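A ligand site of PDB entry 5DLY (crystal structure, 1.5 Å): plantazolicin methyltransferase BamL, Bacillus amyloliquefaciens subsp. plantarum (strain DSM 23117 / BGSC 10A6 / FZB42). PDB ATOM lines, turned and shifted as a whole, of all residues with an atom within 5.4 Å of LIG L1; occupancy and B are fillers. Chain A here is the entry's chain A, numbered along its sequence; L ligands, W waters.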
ATOM      1  N   ALA A  16     -27.277 -24.626  10.838  1.00  0.00           N
ATOM      2  CA  ALA A  16     -27.900 -24.623  12.170  1.00  0.00           C
ATOM      3  C   ALA A  16     -29.413 -24.829  12.060  1.00  0.00           C
ATOM      4  O   ALA A  16     -30.018 -25.534  12.875  1.00  0.00           O
ATOM      5  CB  ALA A  16     -27.600 -23.313  12.890  1.00  0.00           C
ATOM      6  N   PHE A  20     -34.038 -27.705  12.816  1.00  0.00           N
ATOM      7  CA  PHE A  20     -35.425 -27.330  13.060  1.00  0.00           C
ATOM      8  C   PHE A  20     -36.335 -27.631  11.868  1.00  0.00           C
ATOM      9  O   PHE A  20     -37.549 -27.489  11.971  1.00  0.00           O
ATOM     10  CB  PHE A  20     -35.511 -25.867  13.505  1.00  0.00           C
ATOM     11  CG  PHE A  20     -34.755 -25.623  14.772  1.00  0.00           C
ATOM     12  CD1 PHE A  20     -35.338 -25.918  16.003  1.00  0.00           C
ATOM     13  CD2 PHE A  20     -33.435 -25.194  14.740  1.00  0.00           C
ATOM     14  CE1 PHE A  20     -34.635 -25.758  17.177  1.00  0.00           C
ATOM     15  CE2 PHE A  20     -32.730 -25.020  15.914  1.00  0.00           C
ATOM     16  CZ  PHE A  20     -33.333 -25.298  17.134  1.00  0.00           C
ATOM     17  N   TYR A  32     -33.333 -31.432  23.625  1.00  0.00           N
ATOM     18  CA  TYR A  32     -32.313 -30.617  24.263  1.00  0.00           C
ATOM     19  C   TYR A  32     -32.919 -29.297  24.759  1.00  0.00           C
ATOM     20  O   TYR A  32     -32.720 -28.903  25.918  1.00  0.00           O
ATOM     21  CB  TYR A  32     -31.117 -30.323  23.326  1.00  0.00           C
ATOM     22  CG  TYR A  32     -30.089 -29.446  24.010  1.00  0.00           C
ATOM     23  CD1 TYR A  32     -30.222 -28.059  23.988  1.00  0.00           C
ATOM     24  CD2 TYR A  32     -29.022 -30.004  24.714  1.00  0.00           C
ATOM     25  CE1 TYR A  32     -29.312 -27.249  24.648  1.00  0.00           C
ATOM     26  CE2 TYR A  32     -28.096 -29.196  25.376  1.00  0.00           C
ATOM     27  CZ  TYR A  32     -28.250 -27.814  25.331  1.00  0.00           C
ATOM     28  OH  TYR A  32     -27.357 -26.979  25.968  1.00  0.00           O
ATOM     29  N   ASP A  33     -33.650 -28.610  23.872  1.00  0.00           N
ATOM     30  CA  ASP A  33     -34.154 -27.269  24.172  1.00  0.00           C
ATOM     31  C   ASP A  33     -35.115 -27.270  25.350  1.00  0.00           C
ATOM     32  O   ASP A  33     -35.049 -26.397  26.210  1.00  0.00           O
ATOM     33  CB  ASP A  33     -34.838 -26.652  22.951  1.00  0.00           C
ATOM     34  CG  ASP A  33     -33.851 -26.325  21.820  1.00  0.00           C
ATOM     35  OD1 ASP A  33     -32.622 -26.477  22.012  1.00  0.00           O
ATOM     36  OD2 ASP A  33     -34.335 -25.918  20.749  1.00  0.00           O
ATOM     37  N   GLU A  36     -32.907 -28.063  28.627  1.00  0.00           N
ATOM     38  CA  GLU A  36     -31.838 -27.162  29.010  1.00  0.00           C
ATOM     39  C   GLU A  36     -32.170 -25.673  28.919  1.00  0.00           C
ATOM     40  O   GLU A  36     -31.497 -24.855  29.554  1.00  0.00           O
ATOM     41  CB  GLU A  36     -30.563 -27.474  28.197  1.00  0.00           C
ATOM     42  CG  GLU A  36     -30.028 -28.900  28.336  1.00  0.00           C
ATOM     43  CD  GLU A  36     -29.406 -29.229  29.680  1.00  0.00           C
ATOM     44  OE1 GLU A  36     -29.165 -28.318  30.510  1.00  0.00           O
ATOM     45  OE2 GLU A  36     -29.144 -30.414  29.934  1.00  0.00           O
ATOM     46  N   THR A  37     -33.185 -25.322  28.126  1.00  0.00           N
ATOM     47  CA  THR A  37     -33.503 -23.900  27.910  1.00  0.00           C
ATOM     48  C   THR A  37     -34.852 -23.454  28.467  1.00  0.00           C
ATOM     49  O   THR A  37     -35.143 -22.251  28.489  1.00  0.00           O
ATOM     50  CB  THR A  37     -33.377 -23.477  26.416  1.00  0.00           C
ATOM     51  OG1 THR A  37     -34.529 -23.885  25.654  1.00  0.00           O
ATOM     52  CG2 THR A  37     -32.122 -24.044  25.762  1.00  0.00           C
ATOM     53  N   LEU A 131     -33.529 -17.011  21.629  1.00  0.00           N
ATOM     54  CA  LEU A 131     -32.755 -18.207  21.282  1.00  0.00           C
ATOM     55  C   LEU A 131     -32.948 -18.680  19.833  1.00  0.00           C
ATOM     56  O   LEU A 131     -33.036 -19.896  19.553  1.00  0.00           O
ATOM     57  CB  LEU A 131     -32.967 -19.324  22.335  1.00  0.00           C
ATOM     58  CG  LEU A 131     -32.751 -18.948  23.809  1.00  0.00           C
ATOM     59  CD1 LEU A 131     -33.042 -20.116  24.740  1.00  0.00           C
ATOM     60  CD2 LEU A 131     -31.333 -18.420  24.028  1.00  0.00           C
ATOM     61  N   CYS A 132     -32.992 -17.740  18.896  1.00  0.00           N
ATOM     62  CA  CYS A 132     -33.152 -18.117  17.483  1.00  0.00           C
ATOM     63  C   CYS A 132     -32.497 -17.211  16.445  1.00  0.00           C
ATOM     64  O   CYS A 132     -32.533 -17.537  15.255  1.00  0.00           O
ATOM     65  CB  CYS A 132     -34.633 -18.298  17.122  1.00  0.00           C
ATOM     66  SG  CYS A 132     -35.660 -16.826  17.261  1.00  0.00           S
ATOM     67  N   PHE A 133     -31.933 -16.090  16.879  1.00  0.00           N
ATOM     68  CA  PHE A 133     -31.366 -15.085  15.951  1.00  0.00           C
ATOM     69  C   PHE A 133     -30.370 -15.690  14.952  1.00  0.00           C
ATOM     70  O   PHE A 133     -30.437 -15.425  13.747  1.00  0.00           O
ATOM     71  CB  PHE A 133     -30.712 -13.958  16.756  1.00  0.00           C
ATOM     72  CG  PHE A 133     -30.435 -12.709  15.973  1.00  0.00           C
ATOM     73  CD1 PHE A 133     -31.446 -12.045  15.283  1.00  0.00           C
ATOM     74  CD2 PHE A 133     -29.159 -12.174  15.950  1.00  0.00           C
ATOM     75  CE1 PHE A 133     -31.182 -10.888  14.578  1.00  0.00           C
ATOM     76  CE2 PHE A 133     -28.889 -11.003  15.254  1.00  0.00           C
ATOM     77  CZ  PHE A 133     -29.897 -10.353  14.573  1.00  0.00           C
ATOM     78  N   GLY A 134     -29.460 -16.532  15.454  1.00  0.00           N
ATOM     79  CA  GLY A 134     -28.449 -17.197  14.624  1.00  0.00           C
ATOM     80  C   GLY A 134     -28.972 -18.200  13.604  1.00  0.00           C
ATOM     81  O   GLY A 134     -28.191 -18.745  12.822  1.00  0.00           O
ATOM     82  N   LEU A 135     -30.275 -18.467  13.607  1.00  0.00           N
ATOM     83  CA  LEU A 135     -30.881 -19.372  12.615  1.00  0.00           C
ATOM     84  C   LEU A 135     -31.318 -18.650  11.344  1.00  0.00           C
ATOM     85  O   LEU A 135     -31.533 -19.300  10.319  1.00  0.00           O
ATOM     86  CB  LEU A 135     -32.101 -20.105  13.202  1.00  0.00           C
ATOM     87  CG  LEU A 135     -31.835 -20.973  14.436  1.00  0.00           C
ATOM     88  CD1 LEU A 135     -33.147 -21.498  14.985  1.00  0.00           C
ATOM     89  CD2 LEU A 135     -30.926 -22.118  14.024  1.00  0.00           C
ATOM     90  N   ASP A 160     -29.474 -14.685  22.617  1.00  0.00           N
ATOM     91  CA  ASP A 160     -28.945 -15.756  21.797  1.00  0.00           C
ATOM     92  C   ASP A 160     -27.612 -16.276  22.278  1.00  0.00           C
ATOM     93  O   ASP A 160     -26.973 -15.683  23.160  1.00  0.00           O
ATOM     94  CB  ASP A 160     -28.837 -15.309  20.338  1.00  0.00           C
ATOM     95  CG  ASP A 160     -28.952 -16.482  19.332  1.00  0.00           C
ATOM     96  OD1 ASP A 160     -29.438 -17.575  19.716  1.00  0.00           O
ATOM     97  OD2 ASP A 160     -28.578 -16.269  18.155  1.00  0.00           O
ATOM     98  N   LEU A 161     -27.183 -17.397  21.697  1.00  0.00           N
ATOM     99  CA  LEU A 161     -25.867 -17.963  21.957  1.00  0.00           C
ATOM    100  C   LEU A 161     -24.749 -17.030  21.518  1.00  0.00           C
ATOM    101  O   LEU A 161     -24.888 -16.303  20.523  1.00  0.00           O
ATOM    102  CB  LEU A 161     -25.710 -19.271  21.185  1.00  0.00           C
ATOM    103  CG  LEU A 161     -26.705 -20.380  21.479  1.00  0.00           C
ATOM    104  CD1 LEU A 161     -26.422 -21.571  20.561  1.00  0.00           C
ATOM    105  CD2 LEU A 161     -26.643 -20.803  22.933  1.00  0.00           C
ATOM    106  N   GLY A 169     -20.385 -24.557  26.148  1.00  0.00           N
ATOM    107  CA  GLY A 169     -21.730 -24.901  25.693  1.00  0.00           C
ATOM    108  C   GLY A 169     -21.932 -26.379  25.439  1.00  0.00           C
ATOM    109  O   GLY A 169     -23.050 -26.874  25.520  1.00  0.00           O
ATOM    110  N   THR A 172     -23.418 -29.584  28.346  1.00  0.00           N
ATOM    111  CA  THR A 172     -24.777 -30.057  28.608  1.00  0.00           C
ATOM    112  C   THR A 172     -25.302 -31.075  27.589  1.00  0.00           C
ATOM    113  O   THR A 172     -26.406 -31.601  27.738  1.00  0.00           O
ATOM    114  CB  THR A 172     -25.760 -28.878  28.700  1.00  0.00           C
ATOM    115  OG1 THR A 172     -25.525 -27.987  27.617  1.00  0.00           O
ATOM    116  CG2 THR A 172     -25.567 -28.141  30.025  1.00  0.00           C
ATOM    117  N   TYR A 181     -25.489 -31.190  17.269  1.00  0.00           N
ATOM    118  CA  TYR A 181     -26.466 -30.098  17.306  1.00  0.00           C
ATOM    119  C   TYR A 181     -25.866 -28.818  17.870  1.00  0.00           C
ATOM    120  O   TYR A 181     -25.898 -27.773  17.217  1.00  0.00           O
ATOM    121  CB  TYR A 181     -27.666 -30.562  18.130  1.00  0.00           C
ATOM    122  CG  TYR A 181     -28.637 -29.479  18.535  1.00  0.00           C
ATOM    123  CD1 TYR A 181     -29.311 -28.722  17.568  1.00  0.00           C
ATOM    124  CD2 TYR A 181     -28.905 -29.237  19.874  1.00  0.00           C
ATOM    125  CE1 TYR A 181     -30.215 -27.735  17.942  1.00  0.00           C
ATOM    126  CE2 TYR A 181     -29.798 -28.237  20.266  1.00  0.00           C
ATOM    127  CZ  TYR A 181     -30.440 -27.506  19.292  1.00  0.00           C
ATOM    128  OH  TYR A 181     -31.344 -26.526  19.654  1.00  0.00           O
ATOM    129  N   LEU A 182     -25.280 -28.905  19.061  1.00  0.00           N
ATOM    130  CA  LEU A 182     -24.725 -27.719  19.719  1.00  0.00           C
ATOM    131  C   LEU A 182     -23.552 -27.107  18.955  1.00  0.00           C
ATOM    132  O   LEU A 182     -23.445 -25.886  18.854  1.00  0.00           O
ATOM    133  CB  LEU A 182     -24.343 -28.019  21.166  1.00  0.00           C
ATOM    134  CG  LEU A 182     -25.506 -28.304  22.131  1.00  0.00           C
ATOM    135  CD1 LEU A 182     -24.954 -28.593  23.515  1.00  0.00           C
ATOM    136  CD2 LEU A 182     -26.515 -27.156  22.167  1.00  0.00           C
ATOM    137  N   ASP A 184     -23.090 -27.150  15.697  1.00  0.00           N
ATOM    138  CA  ASP A 184     -23.726 -26.405  14.608  1.00  0.00           C
ATOM    139  C   ASP A 184     -24.398 -25.110  15.092  1.00  0.00           C
ATOM    140  O   ASP A 184     -24.289 -24.066  14.446  1.00  0.00           O
ATOM    141  CB  ASP A 184     -24.755 -27.261  13.871  1.00  0.00           C
ATOM    142  CG  ASP A 184     -24.118 -28.255  12.912  1.00  0.00           C
ATOM    143  OD1 ASP A 184     -22.884 -28.177  12.648  1.00  0.00           O
ATOM    144  OD2 ASP A 184     -24.870 -29.097  12.394  1.00  0.00           O
ATOM    145  N   GLN A 185     -25.063 -25.164  16.250  1.00  0.00           N
ATOM    146  CA  GLN A 185     -25.723 -23.972  16.786  1.00  0.00           C
ATOM    147  C   GLN A 185     -24.726 -22.866  17.144  1.00  0.00           C
ATOM    148  O   GLN A 185     -24.917 -21.705  16.785  1.00  0.00           O
ATOM    149  CB  GLN A 185     -26.615 -24.306  17.992  1.00  0.00           C
ATOM    150  CG  GLN A 185     -27.781 -25.250  17.711  1.00  0.00           C
ATOM    151  CD  GLN A 185     -28.542 -24.915  16.439  1.00  0.00           C
ATOM    152  OE1 GLN A 185     -28.702 -25.745  15.540  1.00  0.00           O
ATOM    153  NE2 GLN A 185     -29.007 -23.678  16.350  1.00  0.00           N
ATOM    154  N   TYR A 186     -23.667 -23.223  17.868  1.00  0.00           N
ATOM    155  CA  TYR A 186     -22.649 -22.235  18.239  1.00  0.00           C
ATOM    156  C   TYR A 186     -21.879 -21.675  17.058  1.00  0.00           C
ATOM    157  O   TYR A 186     -21.576 -20.483  17.034  1.00  0.00           O
ATOM    158  CB  TYR A 186     -21.702 -22.755  19.334  1.00  0.00           C
ATOM    159  CG  TYR A 186     -22.332 -22.751  20.715  1.00  0.00           C
ATOM    160  CD1 TYR A 186     -22.315 -21.605  21.510  1.00  0.00           C
ATOM    161  CD2 TYR A 186     -22.964 -23.894  21.203  1.00  0.00           C
ATOM    162  CE1 TYR A 186     -22.894 -21.608  22.774  1.00  0.00           C
ATOM    163  CE2 TYR A 186     -23.559 -23.895  22.465  1.00  0.00           C
ATOM    164  CZ  TYR A 186     -23.523 -22.752  23.238  1.00  0.00           C
ATOM    165  OH  TYR A 186     -24.119 -22.781  24.475  1.00  0.00           O
ATOM    166  N   ALA A 188     -22.977 -21.117  14.140  1.00  0.00           N
ATOM    167  CA  ALA A 188     -23.855 -20.165  13.451  1.00  0.00           C
ATOM    168  C   ALA A 188     -24.023 -18.862  14.218  1.00  0.00           C
ATOM    169  O   ALA A 188     -24.561 -17.884  13.695  1.00  0.00           O
ATOM    170  CB  ALA A 188     -25.218 -20.794  13.196  1.00  0.00           C
ATOM    171  N   SER A 189     -23.570 -18.836  15.475  1.00  0.00           N
ATOM    172  CA  SER A 189     -23.832 -17.692  16.355  1.00  0.00           C
ATOM    173  C   SER A 189     -22.908 -16.508  16.104  1.00  0.00           C
ATOM    174  O   SER A 189     -21.839 -16.661  15.499  1.00  0.00           O
ATOM    175  CB  SER A 189     -23.724 -18.114  17.820  1.00  0.00           C
ATOM    176  OG  SER A 189     -24.534 -19.258  18.061  1.00  0.00           O
ATOM    177  N   MET A 254     -24.431 -22.304  33.199  1.00  0.00           N
ATOM    178  CA  MET A 254     -24.606 -21.921  31.788  1.00  0.00           C
ATOM    179  C   MET A 254     -23.564 -20.919  31.337  1.00  0.00           C
ATOM    180  O   MET A 254     -23.226 -20.015  32.094  1.00  0.00           O
ATOM    181  CB  MET A 254     -25.926 -21.183  31.623  1.00  0.00           C
ATOM    182  CG  MET A 254     -27.175 -22.002  31.609  1.00  0.00           C
ATOM    183  SD  MET A 254     -28.449 -20.827  31.163  1.00  0.00           S
ATOM    184  CE  MET A 254     -29.881 -21.883  31.313  1.00  0.00           C
ATOM    185  N   PRO A 255     -23.097 -21.028  30.076  1.00  0.00           N
ATOM    186  CA  PRO A 255     -22.268 -19.950  29.538  1.00  0.00           C
ATOM    187  C   PRO A 255     -23.091 -18.673  29.399  1.00  0.00           C
ATOM    188  O   PRO A 255     -24.321 -18.722  29.325  1.00  0.00           O
ATOM    189  CB  PRO A 255     -21.884 -20.461  28.140  1.00  0.00           C
ATOM    190  CG  PRO A 255     -22.145 -21.923  28.153  1.00  0.00           C
ATOM    191  CD  PRO A 255     -23.269 -22.135  29.128  1.00  0.00           C
ATOM    192  N   LEU A 257     -24.927 -15.641  27.793  1.00  0.00           N
ATOM    193  CA  LEU A 257     -25.649 -15.454  26.545  1.00  0.00           C
ATOM    194  C   LEU A 257     -25.475 -14.020  26.066  1.00  0.00           C
ATOM    195  O   LEU A 257     -25.135 -13.145  26.865  1.00  0.00           O
ATOM    196  CB  LEU A 257     -27.134 -15.751  26.762  1.00  0.00           C
ATOM    197  CG  LEU A 257     -27.480 -17.216  27.044  1.00  0.00           C
ATOM    198  CD1 LEU A 257     -28.851 -17.339  27.690  1.00  0.00           C
ATOM    199  CD2 LEU A 257     -27.432 -18.034  25.770  1.00  0.00           C
HETATM  200  O1  LIG L   1     -29.893 -21.518  24.896  1.00  0.00           O
HETATM  201  C1  LIG L   1     -29.273 -22.505  24.532  1.00  0.00           C
HETATM  202  O2  LIG L   1     -28.245 -23.087  25.355  1.00  0.00           O
HETATM  203  C2  LIG L   1     -27.808 -22.472  26.567  1.00  0.00           C
HETATM  204  C3  LIG L   1     -29.577 -23.176  23.237  1.00  0.00           C
HETATM  205  N1  LIG L   1     -30.666 -22.843  22.492  1.00  0.00           N
HETATM  206  C4  LIG L   1     -30.808 -23.539  21.359  1.00  0.00           C
HETATM  207  S1  LIG L   1     -29.517 -24.693  21.234  1.00  0.00           S
HETATM  208  C5  LIG L   1     -28.779 -24.211  22.721  1.00  0.00           C
HETATM  209  C6  LIG L   1     -31.846 -23.463  20.308  1.00  0.00           C
HETATM  210  N2  LIG L   1     -32.917 -22.608  20.802  1.00  0.00           N
HETATM  211  C7  LIG L   1     -31.291 -22.941  18.974  1.00  0.00           C
HETATM  212  C8  LIG L   1     -30.332 -21.742  19.078  1.00  0.00           C
HETATM  213  C9  LIG L   1     -30.459 -20.910  17.814  1.00  0.00           C
HETATM  214  N3  LIG L   1     -29.453 -19.854  17.848  1.00  0.00           N
HETATM  215  C10 LIG L   1     -28.191 -19.894  17.425  1.00  0.00           C
HETATM  216  N4  LIG L   1     -27.450 -18.877  17.534  1.00  0.00           N
HETATM  217  N5  LIG L   1     -27.716 -20.951  16.881  1.00  0.00           N
HETATM  218  C11 LIG L   1     -26.681 -23.289  27.140  1.00  0.00           C
HETATM  219  C12 LIG L   1     -26.515 -23.405  28.443  1.00  0.00           C
HETATM  220  N1  LG2 L   2     -38.139 -18.659  20.540  1.00  0.00           N
HETATM  221  C1  LG2 L   2     -38.006 -20.125  20.814  1.00  0.00           C
HETATM  222  C2  LG2 L   2     -36.944 -20.733  19.895  1.00  0.00           C
HETATM  223  C3  LG2 L   2     -37.398 -22.100  19.373  1.00  0.00           C
HETATM  224  S1  LG2 L   2     -36.105 -22.951  18.518  1.00  0.00           S
HETATM  225  C4  LG2 L   2     -37.610 -20.348  22.249  1.00  0.00           C
HETATM  226  O1  LG2 L   2     -37.619 -19.428  23.061  1.00  0.00           O
HETATM  227  O2  LG2 L   2     -37.264 -21.454  22.657  1.00  0.00           O
HETATM  228  C5  LG2 L   2     -35.838 -21.934  17.091  1.00  0.00           C
HETATM  229  C6  LG2 L   2     -37.113 -21.665  16.301  1.00  0.00           C
HETATM  230  O3  LG2 L   2     -36.845 -20.665  15.312  1.00  0.00           O
HETATM  231  C7  LG2 L   2     -37.612 -22.888  15.544  1.00  0.00           C
HETATM  232  O4  LG2 L   2     -38.967 -23.192  15.920  1.00  0.00           O
HETATM  233  C8  LG2 L   2     -37.476 -22.502  14.065  1.00  0.00           C
HETATM  234  O5  LG2 L   2     -38.478 -23.062  13.203  1.00  0.00           O
HETATM  235  C9  LG2 L   2     -37.594 -20.997  14.147  1.00  0.00           C
HETATM  236  N2  LG2 L   2     -37.064 -20.258  12.979  1.00  0.00           N
HETATM  237  C10 LG2 L   2     -35.870 -20.437  12.388  1.00  0.00           C
HETATM  238  N3  LG2 L   2     -35.724 -19.582  11.347  1.00  0.00           N
HETATM  239  C11 LG2 L   2     -36.832 -18.834  11.277  1.00  0.00           C
HETATM  240  C12 LG2 L   2     -37.311 -17.749  10.405  1.00  0.00           C
HETATM  241  N4  LG2 L   2     -36.516 -17.315   9.415  1.00  0.00           N
HETATM  242  N5  LG2 L   2     -38.536 -17.228  10.669  1.00  0.00           N
HETATM  243  C13 LG2 L   2     -39.308 -17.694  11.679  1.00  0.00           C
HETATM  244  N6  LG2 L   2     -38.930 -18.692  12.519  1.00  0.00           N
HETATM  245  C14 LG2 L   2     -37.719 -19.290  12.357  1.00  0.00           C
HETATM  246  O   HOH W   1     -25.332 -25.246  25.232  1.00  0.00           O
HETATM  247  O   HOH W   2     -26.192 -20.335  28.213  1.00  0.00           O
HETATM  248  O   HOH W   3     -27.736 -26.088  28.464  1.00  0.00           O
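N5 of LIG L1 sits at hydrogen-bond distance from O of Gln 185 (2.9 Å). N5 of LIG L1 sits close to NE2 of Gln 185 (3.1 Å). A nitrogen (N4) of LIG L1 is in salt-bridge range of the side-chain carboxylate of Asp 160. OG of Ser 189 lies within hydrogen-bond range of N4 of LIG L1, 3.0 Å away. The backbone carbonyl oxygen of Leu 131 is in hydrogen-bond range of a nitrogen (N2) of LIG L1 (3.0 Å). OH of Tyr 181 sits close to S1 of LIG L1 (3.0 Å). N2 of LIG L1 lies within salt-bridge range of OD2 of Asp 33, 3.6 Å away.
The backbone carbonyl oxygen of Gln 185 sits at hydrogen-bond distance from the side-chain hydroxyl of Ser 189 (2.8 Å). The side-chain amide oxygen (OE1) of Gln 185 lies close to the backbone carbonyl oxygen (O) of Ala 16 (3.0 Å). OD2 of Asp 160 sits at hydrogen-bond distance from N of Gly 134, 2.9 Å away. O of Tyr 186 lies close to OG of Ser 189 (3.4 Å). OH of Tyr 181 is in hydrogen-bond range of OD1 of Asp 33 (2.7 Å). O of Asp 33 sits at hydrogen-bond distance from OG1 of Thr 37, 2.6 Å away. The side-chain hydroxyl (OG1) of Thr 172 sits at hydrogen-bond distance from the side-chain hydroxyl (OH) of Tyr 32 (2.7 Å).
CZ of Phe 20 touches C7 of LIG L1, 3.6 Å away. CE1 of Tyr 32 touches C5 of LIG L1, 3.6 Å away. Thr 37 touches LIG L1 (CG2 to C1, 3.5 Å). Cys 132 touches LIG L1 (CA to C9, 3.9 Å). Gly 134 touches LIG L1 (CA to N4, 3.5 Å). Leu 135 touches LIG L1. Leu 161 touches LIG L1. Leu 182 touches LIG L1 (CD2 to C5, 3.8 Å). Tyr 186 touches LIG L1 (OH to C11, 3.7 Å). Met 254 touches LIG L1 (CG to C12, 3.5 Å). Pro 255 touches LIG L1. Within 4 Å of LIG L1: Phe 20, Tyr 32, Asp 33, Thr 37, Leu 131, Cys 132, Gly 134, Leu 135, Asp 160, Leu 161, Tyr 181, Leu 182, Gln 185, Tyr 186, Ser 189, Met 254 and Pro 255. The nearest printed residue that does not touch LIG L1 is Leu 257 (4.4 Å).
Water W3 lies within hydrogen-bond range of OH of Tyr 32 (2.7 Å), OG1 of Thr 172 (3.0 Å) and OE1 of Glu 36 (3.3 Å). Water W1 lies within hydrogen-bond range of the side-chain hydroxyl (OH) of Tyr 32, the backbone carbonyl oxygen (O) of Gly 169 and the side-chain hydroxyl (OH) of Tyr 186. Water W2 lies within hydrogen-bond range of the backbone carbonyl oxygen of Pro 255 (2.7 Å) and the side-chain sulfur of Met 254 (3.7 Å).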
